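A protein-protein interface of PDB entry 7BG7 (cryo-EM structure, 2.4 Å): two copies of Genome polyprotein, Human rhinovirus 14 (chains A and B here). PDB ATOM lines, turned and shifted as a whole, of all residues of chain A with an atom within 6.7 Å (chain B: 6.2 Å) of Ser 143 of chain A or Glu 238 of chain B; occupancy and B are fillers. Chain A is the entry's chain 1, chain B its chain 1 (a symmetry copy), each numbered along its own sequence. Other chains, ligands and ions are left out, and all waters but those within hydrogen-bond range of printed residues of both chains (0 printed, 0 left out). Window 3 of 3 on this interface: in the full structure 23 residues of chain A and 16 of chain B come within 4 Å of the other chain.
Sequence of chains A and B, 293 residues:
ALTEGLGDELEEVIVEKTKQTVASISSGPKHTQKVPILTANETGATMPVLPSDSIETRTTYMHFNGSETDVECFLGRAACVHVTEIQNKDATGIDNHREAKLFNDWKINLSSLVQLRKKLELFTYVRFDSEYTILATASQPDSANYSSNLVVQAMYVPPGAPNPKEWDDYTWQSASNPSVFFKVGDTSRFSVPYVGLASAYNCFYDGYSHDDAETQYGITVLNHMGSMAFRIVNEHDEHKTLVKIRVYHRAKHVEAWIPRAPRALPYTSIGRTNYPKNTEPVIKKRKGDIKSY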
ATOM      1  N   GLN A 140       3.550  32.787 -17.157  1.00  0.00           N
ATOM      2  CA  GLN A 140       4.847  32.205 -16.819  1.00  0.00           C
ATOM      3  C   GLN A 140       5.787  32.414 -17.997  1.00  0.00           C
ATOM      4  O   GLN A 140       5.991  31.511 -18.815  1.00  0.00           O
ATOM      5  CB  GLN A 140       4.709  30.727 -16.468  1.00  0.00           C
ATOM      6  CG  GLN A 140       3.729  30.463 -15.337  1.00  0.00           C
ATOM      7  CD  GLN A 140       3.692  29.013 -14.925  1.00  0.00           C
ATOM      8  OE1 GLN A 140       3.614  28.696 -13.742  1.00  0.00           O
ATOM      9  NE2 GLN A 140       3.737  28.119 -15.902  1.00  0.00           N
ATOM     10  N   PRO A 141       6.369  33.608 -18.123  1.00  0.00           N
ATOM     11  CA  PRO A 141       7.183  33.889 -19.318  1.00  0.00           C
ATOM     12  C   PRO A 141       8.391  32.977 -19.440  1.00  0.00           C
ATOM     13  O   PRO A 141       8.643  32.421 -20.515  1.00  0.00           O
ATOM     14  CB  PRO A 141       7.582  35.358 -19.128  1.00  0.00           C
ATOM     15  CG  PRO A 141       7.437  35.623 -17.678  1.00  0.00           C
ATOM     16  CD  PRO A 141       6.323  34.753 -17.200  1.00  0.00           C
ATOM     17  N   ASP A 142       9.131  32.786 -18.352  1.00  0.00           N
ATOM     18  CA  ASP A 142      10.296  31.920 -18.373  1.00  0.00           C
ATOM     19  C   ASP A 142       9.877  30.455 -18.433  1.00  0.00           C
ATOM     20  O   ASP A 142       8.696  30.109 -18.363  1.00  0.00           O
ATOM     21  CB  ASP A 142      11.160  32.153 -17.136  1.00  0.00           C
ATOM     22  CG  ASP A 142      11.615  33.585 -17.004  1.00  0.00           C
ATOM     23  OD1 ASP A 142      11.868  34.224 -18.044  1.00  0.00           O
ATOM     24  OD2 ASP A 142      11.719  34.076 -15.862  1.00  0.00           O
ATOM     25  N   SER A 143      10.871  29.588 -18.582  1.00  0.00           N
ATOM     26  CA  SER A 143      10.609  28.161 -18.695  1.00  0.00           C
ATOM     27  C   SER A 143       9.890  27.658 -17.452  1.00  0.00           C
ATOM     28  O   SER A 143      10.356  27.855 -16.328  1.00  0.00           O
ATOM     29  CB  SER A 143      11.915  27.398 -18.898  1.00  0.00           C
ATOM     30  OG  SER A 143      11.667  26.058 -19.277  1.00  0.00           O
ATOM     31  N   ALA A 144       8.747  27.015 -17.661  1.00  0.00           N
ATOM     32  CA  ALA A 144       7.978  26.418 -16.583  1.00  0.00           C
ATOM     33  C   ALA A 144       7.415  25.087 -17.046  1.00  0.00           C
ATOM     34  O   ALA A 144       7.026  24.939 -18.205  1.00  0.00           O
ATOM     35  CB  ALA A 144       6.836  27.328 -16.131  1.00  0.00           C
ATOM     36  N   ASN A 145       7.381  24.121 -16.131  1.00  0.00           N
ATOM     37  CA  ASN A 145       6.935  22.777 -16.466  1.00  0.00           C
ATOM     38  C   ASN A 145       5.425  22.642 -16.402  1.00  0.00           C
ATOM     39  O   ASN A 145       4.880  21.680 -16.943  1.00  0.00           O
ATOM     40  CB  ASN A 145       7.573  21.756 -15.524  1.00  0.00           C
ATOM     41  CG  ASN A 145       9.016  21.478 -15.856  1.00  0.00           C
ATOM     42  OD1 ASN A 145       9.425  21.574 -17.010  1.00  0.00           O
ATOM     43  ND2 ASN A 145       9.798  21.122 -14.848  1.00  0.00           N
ATOM     44  N   GLU A 238       9.262  25.979  -8.409  1.00  0.00           N
ATOM     45  CA  GLU A 238      10.604  25.993  -8.969  1.00  0.00           C
ATOM     46  C   GLU A 238      10.777  27.106  -9.989  1.00  0.00           C
ATOM     47  O   GLU A 238      11.905  27.543 -10.232  1.00  0.00           O
ATOM     48  CB  GLU A 238      10.918  24.642  -9.612  1.00  0.00           C
ATOM     49  CG  GLU A 238      12.387  24.401  -9.867  1.00  0.00           C
ATOM     50  CD  GLU A 238      13.208  24.415  -8.590  1.00  0.00           C
ATOM     51  OE1 GLU A 238      13.520  23.321  -8.074  1.00  0.00           O
ATOM     52  OE2 GLU A 238      13.536  25.519  -8.101  1.00  0.00           O
ATOM     53  N   HIS A 239       9.680  27.569 -10.571  1.00  0.00           N
ATOM     54  CA  HIS A 239       9.649  28.611 -11.579  1.00  0.00           C
ATOM     55  C   HIS A 239       8.932  29.835 -11.024  1.00  0.00           C
ATOM     56  O   HIS A 239       8.293  29.791  -9.972  1.00  0.00           O
ATOM     57  CB  HIS A 239       8.956  28.100 -12.847  1.00  0.00           C
ATOM     58  CG  HIS A 239       7.573  27.579 -12.609  1.00  0.00           C
ATOM     59  ND1 HIS A 239       7.307  26.241 -12.413  1.00  0.00           N
ATOM     60  CD2 HIS A 239       6.380  28.213 -12.536  1.00  0.00           C
ATOM     61  CE1 HIS A 239       6.011  26.075 -12.225  1.00  0.00           C
ATOM     62  NE2 HIS A 239       5.426  27.257 -12.293  1.00  0.00           N
ATOM     63  N   LYS A 240       9.046  30.939 -11.749  1.00  0.00           N
ATOM     64  CA  LYS A 240       8.411  32.195 -11.374  1.00  0.00           C
ATOM     65  C   LYS A 240       7.090  32.352 -12.114  1.00  0.00           C
ATOM     66  O   LYS A 240       7.024  32.136 -13.326  1.00  0.00           O
ATOM     67  CB  LYS A 240       9.334  33.375 -11.683  1.00  0.00           C
ATOM     68  CG  LYS A 240       8.739  34.735 -11.351  1.00  0.00           C
ATOM     69  CD  LYS A 240       9.526  35.872 -11.983  1.00  0.00           C
ATOM     70  CE  LYS A 240      10.923  35.992 -11.386  1.00  0.00           C
ATOM     71  NZ  LYS A 240      11.701  37.084 -12.031  1.00  0.00           N
ATOM     72  N   ASN B 145       4.910  23.013 -22.706  1.00  0.00           N
ATOM     73  CA  ASN B 145       5.090  22.175 -21.531  1.00  0.00           C
ATOM     74  C   ASN B 145       3.790  21.952 -20.781  1.00  0.00           C
ATOM     75  O   ASN B 145       3.714  21.037 -19.960  1.00  0.00           O
ATOM     76  CB  ASN B 145       6.118  22.797 -20.586  1.00  0.00           C
ATOM     77  CG  ASN B 145       7.535  22.619 -21.068  1.00  0.00           C
ATOM     78  OD1 ASN B 145       7.850  21.646 -21.746  1.00  0.00           O
ATOM     79  ND2 ASN B 145       8.403  23.553 -20.710  1.00  0.00           N
ATOM     80  N   TYR B 146       2.770  22.751 -21.057  1.00  0.00           N
ATOM     81  CA  TYR B 146       1.517  22.704 -20.320  1.00  0.00           C
ATOM     82  C   TYR B 146       0.504  23.535 -21.088  1.00  0.00           C
ATOM     83  O   TYR B 146       0.849  24.248 -22.033  1.00  0.00           O
ATOM     84  CB  TYR B 146       1.697  23.231 -18.892  1.00  0.00           C
ATOM     85  CG  TYR B 146       2.193  24.651 -18.866  1.00  0.00           C
ATOM     86  CD1 TYR B 146       3.542  24.935 -19.003  1.00  0.00           C
ATOM     87  CD2 TYR B 146       1.313  25.710 -18.745  1.00  0.00           C
ATOM     88  CE1 TYR B 146       3.998  26.229 -19.002  1.00  0.00           C
ATOM     89  CE2 TYR B 146       1.760  27.004 -18.740  1.00  0.00           C
ATOM     90  CZ  TYR B 146       3.102  27.260 -18.871  1.00  0.00           C
ATOM     91  OH  TYR B 146       3.547  28.556 -18.867  1.00  0.00           O
ATOM     92  N   HIS B 236       2.157  36.963 -21.806  1.00  0.00           N
ATOM     93  CA  HIS B 236       2.664  35.839 -22.575  1.00  0.00           C
ATOM     94  C   HIS B 236       3.288  34.781 -21.675  1.00  0.00           C
ATOM     95  O   HIS B 236       3.870  35.080 -20.630  1.00  0.00           O
ATOM     96  CB  HIS B 236       3.700  36.312 -23.587  1.00  0.00           C
ATOM     97  CG  HIS B 236       4.989  36.743 -22.967  1.00  0.00           C
ATOM     98  ND1 HIS B 236       6.096  35.925 -22.913  1.00  0.00           N
ATOM     99  CD2 HIS B 236       5.343  37.896 -22.354  1.00  0.00           C
ATOM    100  CE1 HIS B 236       7.082  36.562 -22.307  1.00  0.00           C
ATOM    101  NE2 HIS B 236       6.650  37.759 -21.955  1.00  0.00           N
ATOM    102  N   ASP B 237       3.169  33.533 -22.104  1.00  0.00           N
ATOM    103  CA  ASP B 237       3.916  32.434 -21.529  1.00  0.00           C
ATOM    104  C   ASP B 237       5.160  32.193 -22.381  1.00  0.00           C
ATOM    105  O   ASP B 237       5.492  32.984 -23.269  1.00  0.00           O
ATOM    106  CB  ASP B 237       3.039  31.183 -21.460  1.00  0.00           C
ATOM    107  CG  ASP B 237       1.847  31.349 -20.540  1.00  0.00           C
ATOM    108  OD1 ASP B 237       1.585  32.480 -20.089  1.00  0.00           O
ATOM    109  OD2 ASP B 237       1.155  30.341 -20.280  1.00  0.00           O
ATOM    110  N   GLU B 238       5.866  31.099 -22.116  1.00  0.00           N
ATOM    111  CA  GLU B 238       7.063  30.793 -22.884  1.00  0.00           C
ATOM    112  C   GLU B 238       6.725  30.255 -24.264  1.00  0.00           C
ATOM    113  O   GLU B 238       7.547  30.356 -25.179  1.00  0.00           O
ATOM    114  CB  GLU B 238       7.928  29.783 -22.129  1.00  0.00           C
ATOM    115  CG  GLU B 238       9.353  29.694 -22.621  1.00  0.00           C
ATOM    116  CD  GLU B 238      10.098  31.009 -22.487  1.00  0.00           C
ATOM    117  OE1 GLU B 238      10.861  31.162 -21.510  1.00  0.00           O
ATOM    118  OE2 GLU B 238       9.917  31.892 -23.356  1.00  0.00           O
ATOM    119  N   HIS B 239       5.530  29.704 -24.421  1.00  0.00           N
ATOM    120  CA  HIS B 239       5.038  29.121 -25.656  1.00  0.00           C
ATOM    121  C   HIS B 239       3.866  29.943 -26.175  1.00  0.00           C
ATOM    122  O   HIS B 239       3.320  30.803 -25.483  1.00  0.00           O
ATOM    123  CB  HIS B 239       4.625  27.664 -25.425  1.00  0.00           C
ATOM    124  CG  HIS B 239       3.610  27.491 -24.339  1.00  0.00           C
ATOM    125  ND1 HIS B 239       3.955  27.173 -23.043  1.00  0.00           N
ATOM    126  CD2 HIS B 239       2.261  27.590 -24.354  1.00  0.00           C
ATOM    127  CE1 HIS B 239       2.863  27.088 -22.308  1.00  0.00           C
ATOM    128  NE2 HIS B 239       1.821  27.339 -23.078  1.00  0.00           N
ATOM    129  N   LYS B 240       3.480  29.666 -27.413  1.00  0.00           N
ATOM    130  CA  LYS B 240       2.366  30.344 -28.059  1.00  0.00           C
ATOM    131  C   LYS B 240       1.101  29.507 -27.930  1.00  0.00           C
ATOM    132  O   LYS B 240       1.124  28.300 -28.180  1.00  0.00           O
ATOM    133  CB  LYS B 240       2.679  30.606 -29.533  1.00  0.00           C
ATOM    134  CG  LYS B 240       1.554  31.287 -30.299  1.00  0.00           C
ATOM    135  CD  LYS B 240       1.762  31.212 -31.804  1.00  0.00           C
ATOM    136  CE  LYS B 240       2.972  32.024 -32.247  1.00  0.00           C
ATOM    137  NZ  LYS B 240       3.191  31.921 -33.715  1.00  0.00           N
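NE2 of Gln 140 of chain A lies within hydrogen-bond range of OH of Tyr 146 of chain B (3.0 Å). The backbone carbonyl oxygen (O) of Gln 140 of chain A sits at hydrogen-bond distance from the backbone NH (N) of Glu 238 of chain B. The backbone carbonyl oxygen of Pro 141 of chain A lies close to the backbone NH of Glu 238 of chain B (3.5 Å). N of Ser 143 of chain A sits at hydrogen-bond distance from OE1 of Glu 238 of chain B (3.3 Å). O of Ala 144 of chain A is in hydrogen-bond range of ND2 of Asn 145 of chain B. O of Asn 145 of chain B lies close to O of Asn 145 of chain A, at 3.3 Å.
The side-chain amide oxygen (OE1) of Gln 140 of chain A lies within hydrogen-bond range of a ring nitrogen (NE2) of His 239 of chain A, at 2.7 Å. OH of Tyr 146 of chain B lies within hydrogen-bond range of OD2 of Asp 237 of chain B (3.3 Å). The backbone carbonyl oxygen (O) of Tyr 146 of chain B sits at hydrogen-bond distance from a ring nitrogen (NE2) of His 239 of chain B (3.4 Å).
Among the printed residues, merely in contact across the chains: Gln 140 of chain A with Asp 237 of chain B (3.5 Å), Pro 141 of chain A with His 236 of chain B (3.4 Å), Pro 141 of chain A with Asp 237 of chain B (3.96 Å), Asp 142 of chain A with Glu 238 of chain B (3.3 Å), Ala 144 of chain A with Tyr 146 of chain B (3.4 Å) and Asn 145 of chain A with Tyr 146 of chain B (3.9 Å).
Printed residues of chain B within 4 Å of Ser 143 of chain A: Glu 238 (3.3 Å). Of the printed residues of chain A, Glu 238 of chain B touches Gln 140 (3.3 Å), Pro 141 (2.7 Å), Asp 142 (3.3 Å) and Ser 143 (3.3 Å). Of the printed residues of chain B, Ala 144 of chain A touches Asn 145 (3.2 Å) and Tyr 146 (3.4 Å). Printed residues of chain B within 4 Å of Gln 140 of chain A: Tyr 146, Asp 237 and Glu 238. Of the printed residues of chain B, Asn 145 of chain A touches Asn 145 (3.3 Å) and Tyr 146 (3.9 Å). Of the printed residues of chain B, Asp 142 of chain A touches Glu 238 (3.3 Å). Of the printed residues of chain A, Asn 145 of chain B touches Ala 144 and Asn 145. His 239 of chain B touches none of the printed residues of chain A. Lys 240 of chain A touches none of the printed residues of chain B. The nearest residue of chain B that does not touch Ser 143 of chain A is Asn 145 of chain B (4.4 Å). The nearest printed residue of chain A that does not touch Asn 145 of chain B is Ser 143 of chain A (4.4 Å).
Of the 7 printed residues of chain B, 5 touch a printed residue of chain A. Printed residues of chain B that touch a printed residue of chain A: Asn 145, Tyr 146, His 236, Asp 237 and Glu 238. Among the printed residues, no Asp or Glu carboxylate lies within 4 Å of a Lys or Arg side-chain nitrogen of the other chain.
Asn 145 of chain B touches its own counterpart, Asn 145 of chain A. Of the 12 pairs that touch across the chains among the printed residues, 1 has its exchanged pair printed and touching as well.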
